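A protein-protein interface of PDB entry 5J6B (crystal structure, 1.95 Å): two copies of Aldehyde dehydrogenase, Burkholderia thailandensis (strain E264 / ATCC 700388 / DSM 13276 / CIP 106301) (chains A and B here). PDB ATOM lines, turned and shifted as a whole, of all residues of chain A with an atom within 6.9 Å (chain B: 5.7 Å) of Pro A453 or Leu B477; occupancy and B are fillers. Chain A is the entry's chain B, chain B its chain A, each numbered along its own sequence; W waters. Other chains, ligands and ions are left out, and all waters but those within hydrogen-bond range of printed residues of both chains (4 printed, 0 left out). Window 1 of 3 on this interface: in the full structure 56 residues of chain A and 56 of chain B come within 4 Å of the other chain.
Of the printed residues of chain B, Gly A438 touches Leu B479. Of chain B, only Leu B477 (3.97 Å) and Leu B479 (3.4 Å) come within 4 Å of Pro A453. Tyr B147 touches none of the printed residues of chain A. Leu B477 touches just these residues of chain A: Gly A437 (3.7 Å), Pro A453 (3.97 Å) and Arg A464 (2.9 Å). Of the printed residues of chain A, Leu B479 touches Gly A437, Gly A438, Met A452 and Pro A453.
Gly A437 touches Leu B477. Gly A437 touches Arg B478. Gly A438 touches Leu B479. Met A452 touches Leu B479. Pro A453 touches Leu B477 (CB to CD1, 3.97 Å). Leu B479 touches Pro A453 (CD2 to O, 3.4 Å). CG1 of Val A457 touches CD of Glu B476 (3.8 Å).
No position is printed for both chains.
O of Lys B148 lies within hydrogen-bond range of N of Arg B478 (2.8 Å). N of Glu B476 sits at hydrogen-bond distance from O of Val B150 (2.8 Å). N of Val A449 lies within hydrogen-bond range of SD of Met A452.
Water W2 lies within hydrogen-bond range of the backbone carbonyl oxygen (O) of Val A436 (2.6 Å), the backbone carbonyl oxygen (O) of Leu B477 (2.8 Å) and the guanidinium group (NE) of Arg B478 (3.1 Å). Water W3 lies within hydrogen-bond range of OE1 of Glu B476 (2.7 Å), N of Leu B477 (2.9 Å) and NH2 of Arg A464 (3.5 Å). Water W4 lies within hydrogen-bond range of OE2 of Glu B476 (2.9 Å) and NH1 of Arg A464 (2.9 Å). Water W1 lies within hydrogen-bond range of NE of Arg A464 (2.9 Å), O of Gly A437 (2.9 Å) and O of Leu B477 (3.2 Å).
Hydrophobic or aromatic side chains of chain A within 4 Å of the printed part of chain B: Met A452, Pro A453 and Val A457. Among the printed residues, 11 pairs touch across the chains. Among the printed residues, Asp or Glu carboxylates within 4 Å of a Lys or Arg side-chain nitrogen of the other chain: Arg A464 with Glu B476 (2.9 Å).
The guanidinium group of Arg A464 lies within hydrogen-bond range of the backbone carbonyl oxygen of Leu B477. OE1 of Glu B476 is in salt-bridge range of NH2 of Arg A464. N of Leu B479 lies within hydrogen-bond range of O of Gly A437 (3.0 Å). NE of Arg B478 is in hydrogen-bond range of O of Val A436, 3.3 Å away.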
ATOM      1  N   GLU A 257     -27.529   2.507 -29.879  1.00  0.00           N
ATOM      2  CA  GLU A 257     -26.922   3.431 -28.924  1.00  0.00           C
ATOM      3  C   GLU A 257     -27.200   4.818 -29.474  1.00  0.00           C
ATOM      4  O   GLU A 257     -26.586   5.227 -30.466  1.00  0.00           O
ATOM      5  CB  GLU A 257     -25.421   3.172 -28.771  1.00  0.00           C
ATOM      6  CG  GLU A 257     -25.078   1.911 -28.004  1.00  0.00           C
ATOM      7  CD  GLU A 257     -25.239   2.060 -26.494  1.00  0.00           C
ATOM      8  OE1 GLU A 257     -25.578   3.160 -26.022  1.00  0.00           O
ATOM      9  OE2 GLU A 257     -25.012   1.060 -25.780  1.00  0.00           O
ATOM     10  N   GLN A 416     -28.415   8.877 -19.649  1.00  0.00           N
ATOM     11  CA  GLN A 416     -27.868   8.992 -18.303  1.00  0.00           C
ATOM     12  C   GLN A 416     -28.316  10.303 -17.675  1.00  0.00           C
ATOM     13  O   GLN A 416     -28.679  11.266 -18.366  1.00  0.00           O
ATOM     14  CB  GLN A 416     -26.326   8.870 -18.296  1.00  0.00           C
ATOM     15  CG  GLN A 416     -25.871   7.499 -18.816  1.00  0.00           C
ATOM     16  CD  GLN A 416     -24.416   7.143 -18.554  1.00  0.00           C
ATOM     17  OE1 GLN A 416     -24.051   5.972 -18.639  1.00  0.00           O
ATOM     18  NE2 GLN A 416     -23.582   8.138 -18.253  1.00  0.00           N
ATOM     19  N   VAL A 436     -33.487   6.112 -16.796  1.00  0.00           N
ATOM     20  CA  VAL A 436     -32.295   6.237 -17.626  1.00  0.00           C
ATOM     21  C   VAL A 436     -31.533   4.924 -17.558  1.00  0.00           C
ATOM     22  O   VAL A 436     -31.743   4.098 -16.662  1.00  0.00           O
ATOM     23  CB  VAL A 436     -31.376   7.399 -17.179  1.00  0.00           C
ATOM     24  CG1 VAL A 436     -32.071   8.733 -17.369  1.00  0.00           C
ATOM     25  CG2 VAL A 436     -30.966   7.213 -15.713  1.00  0.00           C
ATOM     26  N   GLY A 437     -30.624   4.736 -18.516  1.00  0.00           N
ATOM     27  CA  GLY A 437     -29.735   3.592 -18.430  1.00  0.00           C
ATOM     28  C   GLY A 437     -28.834   3.663 -17.210  1.00  0.00           C
ATOM     29  O   GLY A 437     -28.639   2.663 -16.512  1.00  0.00           O
ATOM     30  N   GLY A 438     -28.294   4.854 -16.924  1.00  0.00           N
ATOM     31  CA  GLY A 438     -27.325   5.024 -15.858  1.00  0.00           C
ATOM     32  C   GLY A 438     -27.474   6.310 -15.058  1.00  0.00           C
ATOM     33  O   GLY A 438     -27.636   7.389 -15.623  1.00  0.00           O
ATOM     34  N   ARG A 448     -18.336   8.270 -18.421  1.00  0.00           N
ATOM     35  CA  ARG A 448     -18.382   6.877 -18.826  1.00  0.00           C
ATOM     36  C   ARG A 448     -16.997   6.274 -18.671  1.00  0.00           C
ATOM     37  O   ARG A 448     -15.995   6.907 -19.018  1.00  0.00           O
ATOM     38  CB  ARG A 448     -18.854   6.714 -20.274  1.00  0.00           C
ATOM     39  CG  ARG A 448     -18.919   5.261 -20.731  1.00  0.00           C
ATOM     40  CD  ARG A 448     -19.209   5.160 -22.240  1.00  0.00           C
ATOM     41  NE  ARG A 448     -19.381   3.774 -22.671  1.00  0.00           N
ATOM     42  CZ  ARG A 448     -19.679   3.398 -23.911  1.00  0.00           C
ATOM     43  NH1 ARG A 448     -19.792   4.312 -24.878  1.00  0.00           N
ATOM     44  NH2 ARG A 448     -19.848   2.106 -24.194  1.00  0.00           N
ATOM     45  N   VAL A 449     -16.948   5.053 -18.151  1.00  0.00           N
ATOM     46  CA  VAL A 449     -15.742   4.241 -18.207  1.00  0.00           C
ATOM     47  C   VAL A 449     -16.067   3.026 -19.065  1.00  0.00           C
ATOM     48  O   VAL A 449     -17.208   2.550 -19.102  1.00  0.00           O
ATOM     49  CB  VAL A 449     -15.225   3.872 -16.791  1.00  0.00           C
ATOM     50  CG1 VAL A 449     -16.217   2.983 -16.041  1.00  0.00           C
ATOM     51  CG2 VAL A 449     -13.809   3.274 -16.847  1.00  0.00           C
ATOM     52  N   ASP A 450     -15.071   2.564 -19.820  1.00  0.00           N
ATOM     53  CA  ASP A 450     -15.387   1.719 -20.960  1.00  0.00           C
ATOM     54  C   ASP A 450     -15.679   0.257 -20.616  1.00  0.00           C
ATOM     55  O   ASP A 450     -15.996  -0.510 -21.527  1.00  0.00           O
ATOM     56  CB  ASP A 450     -14.256   1.835 -21.982  1.00  0.00           C
ATOM     57  CG  ASP A 450     -14.161   3.233 -22.541  1.00  0.00           C
ATOM     58  OD1 ASP A 450     -13.217   3.951 -22.171  1.00  0.00           O
ATOM     59  OD2 ASP A 450     -15.072   3.633 -23.312  1.00  0.00           O
ATOM     60  N   ASN A 451     -15.608  -0.163 -19.345  1.00  0.00           N
ATOM     61  CA  ASN A 451     -16.095  -1.498 -19.011  1.00  0.00           C
ATOM     62  C   ASN A 451     -17.531  -1.504 -18.495  1.00  0.00           C
ATOM     63  O   ASN A 451     -18.106  -2.584 -18.323  1.00  0.00           O
ATOM     64  CB  ASN A 451     -15.192  -2.157 -17.959  1.00  0.00           C
ATOM     65  CG  ASN A 451     -15.169  -1.377 -16.673  1.00  0.00           C
ATOM     66  OD1 ASN A 451     -15.309  -0.155 -16.687  1.00  0.00           O
ATOM     67  ND2 ASN A 451     -15.017  -2.071 -15.550  1.00  0.00           N
ATOM     68  N   MET A 452     -18.123  -0.336 -18.237  1.00  0.00           N
ATOM     69  CA  MET A 452     -19.410  -0.318 -17.550  1.00  0.00           C
ATOM     70  C   MET A 452     -20.560  -0.547 -18.532  1.00  0.00           C
ATOM     71  O   MET A 452     -20.470  -0.164 -19.706  1.00  0.00           O
ATOM     72  CB  MET A 452     -19.603   1.014 -16.817  1.00  0.00           C
ATOM     73  CG  MET A 452     -20.089   2.193 -17.690  1.00  0.00           C
ATOM     74  SD  MET A 452     -19.962   3.775 -16.816  1.00  0.00           S
ATOM     75  CE  MET A 452     -21.243   4.748 -17.625  1.00  0.00           C
ATOM     76  N   PRO A 453     -21.656  -1.169 -18.079  1.00  0.00           N
ATOM     77  CA  PRO A 453     -22.824  -1.289 -18.952  1.00  0.00           C
ATOM     78  C   PRO A 453     -23.283   0.110 -19.317  1.00  0.00           C
ATOM     79  O   PRO A 453     -23.417   0.976 -18.450  1.00  0.00           O
ATOM     80  CB  PRO A 453     -23.859  -2.023 -18.086  1.00  0.00           C
ATOM     81  CG  PRO A 453     -23.502  -1.637 -16.681  1.00  0.00           C
ATOM     82  CD  PRO A 453     -21.965  -1.541 -16.688  1.00  0.00           C
ATOM     83  N   TYR A 454     -23.499   0.334 -20.610  1.00  0.00           N
ATOM     84  CA  TYR A 454     -23.740   1.680 -21.110  1.00  0.00           C
ATOM     85  C   TYR A 454     -24.824   1.648 -22.178  1.00  0.00           C
ATOM     86  O   TYR A 454     -24.709   0.899 -23.153  1.00  0.00           O
ATOM     87  CB  TYR A 454     -22.452   2.303 -21.691  1.00  0.00           C
ATOM     88  CG  TYR A 454     -22.726   3.668 -22.299  1.00  0.00           C
ATOM     89  CD1 TYR A 454     -22.890   4.791 -21.492  1.00  0.00           C
ATOM     90  CD2 TYR A 454     -22.895   3.818 -23.672  1.00  0.00           C
ATOM     91  CE1 TYR A 454     -23.174   6.041 -22.054  1.00  0.00           C
ATOM     92  CE2 TYR A 454     -23.187   5.053 -24.237  1.00  0.00           C
ATOM     93  CZ  TYR A 454     -23.319   6.159 -23.426  1.00  0.00           C
ATOM     94  OH  TYR A 454     -23.599   7.384 -24.000  1.00  0.00           O
ATOM     95  N   GLY A 455     -25.849   2.475 -22.020  1.00  0.00           N
ATOM     96  CA  GLY A 455     -26.890   2.551 -23.026  1.00  0.00           C
ATOM     97  C   GLY A 455     -28.096   3.297 -22.496  1.00  0.00           C
ATOM     98  O   GLY A 455     -28.141   3.722 -21.338  1.00  0.00           O
ATOM     99  N   VAL A 457     -32.576   3.921 -22.266  1.00  0.00           N
ATOM    100  CA  VAL A 457     -33.944   3.436 -22.388  1.00  0.00           C
ATOM    101  C   VAL A 457     -34.751   4.547 -23.057  1.00  0.00           C
ATOM    102  O   VAL A 457     -34.175   5.530 -23.540  1.00  0.00           O
ATOM    103  CB  VAL A 457     -34.538   3.023 -21.020  1.00  0.00           C
ATOM    104  CG1 VAL A 457     -33.846   1.752 -20.492  1.00  0.00           C
ATOM    105  CG2 VAL A 457     -34.417   4.144 -20.010  1.00  0.00           C
ATOM    106  N   ARG A 464     -27.129  -2.694 -24.365  1.00  0.00           N
ATOM    107  CA  ARG A 464     -26.006  -2.117 -23.632  1.00  0.00           C
ATOM    108  C   ARG A 464     -24.697  -2.442 -24.329  1.00  0.00           C
ATOM    109  O   ARG A 464     -24.499  -3.559 -24.815  1.00  0.00           O
ATOM    110  CB  ARG A 464     -25.921  -2.629 -22.177  1.00  0.00           C
ATOM    111  CG  ARG A 464     -27.109  -2.242 -21.291  1.00  0.00           C
ATOM    112  CD  ARG A 464     -27.201  -0.733 -21.054  1.00  0.00           C
ATOM    113  NE  ARG A 464     -28.335  -0.458 -20.178  1.00  0.00           N
ATOM    114  CZ  ARG A 464     -29.591  -0.317 -20.594  1.00  0.00           C
ATOM    115  NH1 ARG A 464     -29.880  -0.373 -21.893  1.00  0.00           N
ATOM    116  NH2 ARG A 464     -30.559  -0.109 -19.704  1.00  0.00           N
ATOM    117  N   GLU A 465     -23.806  -1.457 -24.370  1.00  0.00           N
ATOM    118  CA  GLU A 465     -22.417  -1.666 -24.723  1.00  0.00           C
ATOM    119  C   GLU A 465     -21.591  -1.579 -23.450  1.00  0.00           C
ATOM    120  O   GLU A 465     -22.133  -1.614 -22.336  1.00  0.00           O
ATOM    121  CB  GLU A 465     -21.980  -0.673 -25.805  1.00  0.00           C
ATOM    122  CG  GLU A 465     -22.456  -1.140 -27.172  1.00  0.00           C
ATOM    123  CD  GLU A 465     -22.045  -0.240 -28.324  1.00  0.00           C
ATOM    124  OE1 GLU A 465     -22.239  -0.667 -29.481  1.00  0.00           O
ATOM    125  OE2 GLU A 465     -21.548   0.880 -28.089  1.00  0.00           O
ATOM    126  N   GLY A 466     -20.277  -1.459 -23.610  1.00  0.00           N
ATOM    127  CA  GLY A 466     -19.381  -1.859 -22.550  1.00  0.00           C
ATOM    128  C   GLY A 466     -19.025  -3.302 -22.822  1.00  0.00           C
ATOM    129  O   GLY A 466     -19.915  -4.104 -23.130  1.00  0.00           O
ATOM    130  N   ILE A 467     -17.730  -3.634 -22.742  1.00  0.00           N
ATOM    131  CA  ILE A 467     -17.201  -4.810 -23.443  1.00  0.00           C
ATOM    132  C   ILE A 467     -18.033  -6.060 -23.144  1.00  0.00           C
ATOM    133  O   ILE A 467     -18.519  -6.733 -24.060  1.00  0.00           O
ATOM    134  CB  ILE A 467     -15.720  -5.022 -23.090  1.00  0.00           C
ATOM    135  CG1 ILE A 467     -14.863  -3.892 -23.686  1.00  0.00           C
ATOM    136  CG2 ILE A 467     -15.255  -6.375 -23.581  1.00  0.00           C
ATOM    137  CD1 ILE A 467     -15.082  -3.675 -25.195  1.00  0.00           C
ATOM    138  N   ARG A 468     -18.202  -6.385 -21.852  1.00  0.00           N
ATOM    139  CA  ARG A 468     -18.894  -7.615 -21.454  1.00  0.00           C
ATOM    140  C   ARG A 468     -20.316  -7.654 -21.986  1.00  0.00           C
ATOM    141  O   ARG A 468     -20.818  -8.709 -22.389  1.00  0.00           O
ATOM    142  CB  ARG A 468     -18.941  -7.720 -19.925  1.00  0.00           C
ATOM    143  CG  ARG A 468     -18.090  -8.789 -19.294  1.00  0.00           C
ATOM    144  CD  ARG A 468     -18.772  -9.335 -18.030  1.00  0.00           C
ATOM    145  NE  ARG A 468     -19.314  -8.281 -17.170  1.00  0.00           N
ATOM    146  CZ  ARG A 468     -20.345  -8.444 -16.337  1.00  0.00           C
ATOM    147  NH1 ARG A 468     -20.774  -7.432 -15.586  1.00  0.00           N
ATOM    148  NH2 ARG A 468     -20.962  -9.619 -16.261  1.00  0.00           N
ATOM    149  N   TYR A 469     -21.000  -6.517 -21.936  1.00  0.00           N
ATOM    150  CA  TYR A 469     -22.396  -6.440 -22.334  1.00  0.00           C
ATOM    151  C   TYR A 469     -22.531  -6.486 -23.844  1.00  0.00           C
ATOM    152  O   TYR A 469     -23.471  -7.099 -24.358  1.00  0.00           O
ATOM    153  CB  TYR A 469     -23.005  -5.173 -21.717  1.00  0.00           C
ATOM    154  CG  TYR A 469     -22.598  -5.112 -20.257  1.00  0.00           C
ATOM    155  CD1 TYR A 469     -21.451  -4.411 -19.854  1.00  0.00           C
ATOM    156  CD2 TYR A 469     -23.294  -5.836 -19.299  1.00  0.00           C
ATOM    157  CE1 TYR A 469     -21.040  -4.411 -18.530  1.00  0.00           C
ATOM    158  CE2 TYR A 469     -22.897  -5.834 -17.968  1.00  0.00           C
ATOM    159  CZ  TYR A 469     -21.771  -5.121 -17.590  1.00  0.00           C
ATOM    160  OH  TYR A 469     -21.377  -5.127 -16.268  1.00  0.00           O
ATOM    161  N   GLU A 472     -22.171 -10.156 -24.905  1.00  0.00           N
ATOM    162  CA  GLU A 472     -23.423 -10.884 -24.686  1.00  0.00           C
ATOM    163  C   GLU A 472     -24.352 -10.760 -25.881  1.00  0.00           C
ATOM    164  O   GLU A 472     -24.997 -11.726 -26.296  1.00  0.00           O
ATOM    165  CB  GLU A 472     -24.139 -10.349 -23.444  1.00  0.00           C
ATOM    166  CG  GLU A 472     -23.562 -10.782 -22.110  1.00  0.00           C
ATOM    167  CD  GLU A 472     -24.466 -10.388 -20.951  1.00  0.00           C
ATOM    168  OE1 GLU A 472     -25.659 -10.098 -21.207  1.00  0.00           O
ATOM    169  OE2 GLU A 472     -23.985 -10.362 -19.794  1.00  0.00           O
ATOM    170  N   VAL B 132     -19.824  -3.481 -10.004  1.00  0.00           N
ATOM    171  CA  VAL B 132     -18.840  -3.385 -11.077  1.00  0.00           C
ATOM    172  C   VAL B 132     -17.668  -2.572 -10.554  1.00  0.00           C
ATOM    173  O   VAL B 132     -17.865  -1.466 -10.042  1.00  0.00           O
ATOM    174  CB  VAL B 132     -19.418  -2.709 -12.340  1.00  0.00           C
ATOM    175  CG1 VAL B 132     -18.478  -2.903 -13.526  1.00  0.00           C
ATOM    176  CG2 VAL B 132     -20.809  -3.213 -12.665  1.00  0.00           C
ATOM    177  N   TYR B 147     -25.444  -2.109 -10.222  1.00  0.00           N
ATOM    178  CA  TYR B 147     -26.566  -2.166 -11.149  1.00  0.00           C
ATOM    179  C   TYR B 147     -27.642  -3.100 -10.612  1.00  0.00           C
ATOM    180  O   TYR B 147     -27.352  -4.093  -9.943  1.00  0.00           O
ATOM    181  CB  TYR B 147     -26.132  -2.589 -12.577  1.00  0.00           C
ATOM    182  CG  TYR B 147     -25.610  -4.008 -12.686  1.00  0.00           C
ATOM    183  CD1 TYR B 147     -26.482  -5.079 -12.886  1.00  0.00           C
ATOM    184  CD2 TYR B 147     -24.250  -4.280 -12.594  1.00  0.00           C
ATOM    185  CE1 TYR B 147     -26.009  -6.379 -12.976  1.00  0.00           C
ATOM    186  CE2 TYR B 147     -23.769  -5.576 -12.689  1.00  0.00           C
ATOM    187  CZ  TYR B 147     -24.652  -6.619 -12.880  1.00  0.00           C
ATOM    188  OH  TYR B 147     -24.177  -7.908 -12.974  1.00  0.00           O
ATOM    189  N   LYS B 148     -28.891  -2.761 -10.899  1.00  0.00           N
ATOM    190  CA  LYS B 148     -30.018  -3.631 -10.604  1.00  0.00           C
ATOM    191  C   LYS B 148     -30.898  -3.685 -11.839  1.00  0.00           C
ATOM    192  O   LYS B 148     -30.801  -2.836 -12.726  1.00  0.00           O
ATOM    193  CB  LYS B 148     -30.820  -3.137  -9.389  1.00  0.00           C
ATOM    194  CG  LYS B 148     -31.448  -1.766  -9.573  1.00  0.00           C
ATOM    195  CD  LYS B 148     -32.171  -1.319  -8.299  1.00  0.00           C
ATOM    196  CE  LYS B 148     -32.640   0.122  -8.379  1.00  0.00           C
ATOM    197  NZ  LYS B 148     -33.260   0.546  -7.087  1.00  0.00           N
ATOM    198  N   ARG B 149     -31.769  -4.685 -11.887  1.00  0.00           N
ATOM    199  CA  ARG B 149     -32.700  -4.851 -12.993  1.00  0.00           C
ATOM    200  C   ARG B 149     -34.044  -4.244 -12.620  1.00  0.00           C
ATOM    201  O   ARG B 149     -34.535  -4.449 -11.505  1.00  0.00           O
ATOM    202  CB  ARG B 149     -32.854  -6.331 -13.341  1.00  0.00           C
ATOM    203  CG  ARG B 149     -31.571  -6.953 -13.742  1.00  0.00           C
ATOM    204  CD  ARG B 149     -31.754  -8.400 -14.142  1.00  0.00           C
ATOM    205  NE  ARG B 149     -30.663  -8.846 -15.003  1.00  0.00           N
ATOM    206  CZ  ARG B 149     -30.584  -8.562 -16.299  1.00  0.00           C
ATOM    207  NH1 ARG B 149     -31.533  -7.829 -16.888  1.00  0.00           N
ATOM    208  NH2 ARG B 149     -29.560  -9.011 -17.008  1.00  0.00           N
ATOM    209  N   VAL B 150     -34.615  -3.472 -13.534  1.00  0.00           N
ATOM    210  CA  VAL B 150     -35.922  -2.852 -13.329  1.00  0.00           C
ATOM    211  C   VAL B 150     -36.837  -3.343 -14.441  1.00  0.00           C
ATOM    212  O   VAL B 150     -36.362  -3.805 -15.489  1.00  0.00           O
ATOM    213  CB  VAL B 150     -35.829  -1.309 -13.291  1.00  0.00           C
ATOM    214  CG1 VAL B 150     -35.031  -0.852 -12.081  1.00  0.00           C
ATOM    215  CG2 VAL B 150     -35.237  -0.765 -14.602  1.00  0.00           C
ATOM    216  N   THR B 475     -36.528  -7.114 -18.311  1.00  0.00           N
ATOM    217  CA  THR B 475     -35.957  -6.141 -17.397  1.00  0.00           C
ATOM    218  C   THR B 475     -34.846  -5.368 -18.098  1.00  0.00           C
ATOM    219  O   THR B 475     -34.267  -5.829 -19.081  1.00  0.00           O
ATOM    220  CB  THR B 475     -35.412  -6.799 -16.116  1.00  0.00           C
ATOM    221  OG1 THR B 475     -34.487  -7.837 -16.460  1.00  0.00           O
ATOM    222  CG2 THR B 475     -36.553  -7.371 -15.272  1.00  0.00           C
ATOM    223  N   GLU B 476     -34.563  -4.173 -17.585  1.00  0.00           N
ATOM    224  CA  GLU B 476     -33.444  -3.362 -18.053  1.00  0.00           C
ATOM    225  C   GLU B 476     -32.438  -3.186 -16.928  1.00  0.00           C
ATOM    226  O   GLU B 476     -32.819  -3.021 -15.764  1.00  0.00           O
ATOM    227  CB  GLU B 476     -33.912  -1.970 -18.532  1.00  0.00           C
ATOM    228  CG  GLU B 476     -34.657  -1.979 -19.864  1.00  0.00           C
ATOM    229  CD  GLU B 476     -33.716  -2.021 -21.063  1.00  0.00           C
ATOM    230  OE1 GLU B 476     -32.483  -1.997 -20.862  1.00  0.00           O
ATOM    231  OE2 GLU B 476     -34.207  -2.076 -22.206  1.00  0.00           O
ATOM    232  N   LEU B 477     -31.153  -3.183 -17.277  1.00  0.00           N
ATOM    233  CA  LEU B 477     -30.150  -2.774 -16.304  1.00  0.00           C
ATOM    234  C   LEU B 477     -30.294  -1.292 -15.982  1.00  0.00           C
ATOM    235  O   LEU B 477     -30.494  -0.462 -16.868  1.00  0.00           O
ATOM    236  CB  LEU B 477     -28.740  -3.050 -16.825  1.00  0.00           C
ATOM    237  CG  LEU B 477     -28.313  -4.505 -16.997  1.00  0.00           C
ATOM    238  CD1 LEU B 477     -26.813  -4.572 -17.348  1.00  0.00           C
ATOM    239  CD2 LEU B 477     -28.590  -5.283 -15.742  1.00  0.00           C
ATOM    240  N   ARG B 478     -30.202  -0.966 -14.697  1.00  0.00           N
ATOM    241  CA  ARG B 478     -30.187   0.409 -14.207  1.00  0.00           C
ATOM    242  C   ARG B 478     -28.886   0.548 -13.414  1.00  0.00           C
ATOM    243  O   ARG B 478     -28.762   0.031 -12.296  1.00  0.00           O
ATOM    244  CB  ARG B 478     -31.439   0.697 -13.375  1.00  0.00           C
ATOM    245  CG  ARG B 478     -31.444   1.999 -12.594  1.00  0.00           C
ATOM    246  CD  ARG B 478     -32.059   3.188 -13.336  1.00  0.00           C
ATOM    247  NE  ARG B 478     -33.312   2.927 -14.055  1.00  0.00           N
ATOM    248  CZ  ARG B 478     -34.548   3.075 -13.566  1.00  0.00           C
ATOM    249  NH1 ARG B 478     -34.766   3.450 -12.308  1.00  0.00           N
ATOM    250  NH2 ARG B 478     -35.588   2.847 -14.357  1.00  0.00           N
ATOM    251  N   LEU B 479     -27.905   1.214 -14.014  1.00  0.00           N
ATOM    252  CA  LEU B 479     -26.579   1.365 -13.432  1.00  0.00           C
ATOM    253  C   LEU B 479     -26.548   2.594 -12.536  1.00  0.00           C
ATOM    254  O   LEU B 479     -27.114   3.639 -12.877  1.00  0.00           O
ATOM    255  CB  LEU B 479     -25.521   1.503 -14.538  1.00  0.00           C
ATOM    256  CG  LEU B 479     -24.099   1.889 -14.111  1.00  0.00           C
ATOM    257  CD1 LEU B 479     -23.403   0.745 -13.380  1.00  0.00           C
ATOM    258  CD2 LEU B 479     -23.270   2.365 -15.316  1.00  0.00           C
HETATM  259  O   HOH W   1     -27.435   0.228 -17.543  1.00  0.00           O
HETATM  260  O   HOH W   2     -32.428   1.611 -16.714  1.00  0.00           O
HETATM  261  O   HOH W   3     -30.423  -3.578 -20.033  1.00  0.00           O
HETATM  262  O   HOH W   4     -32.257  -0.496 -23.582  1.00  0.00           O
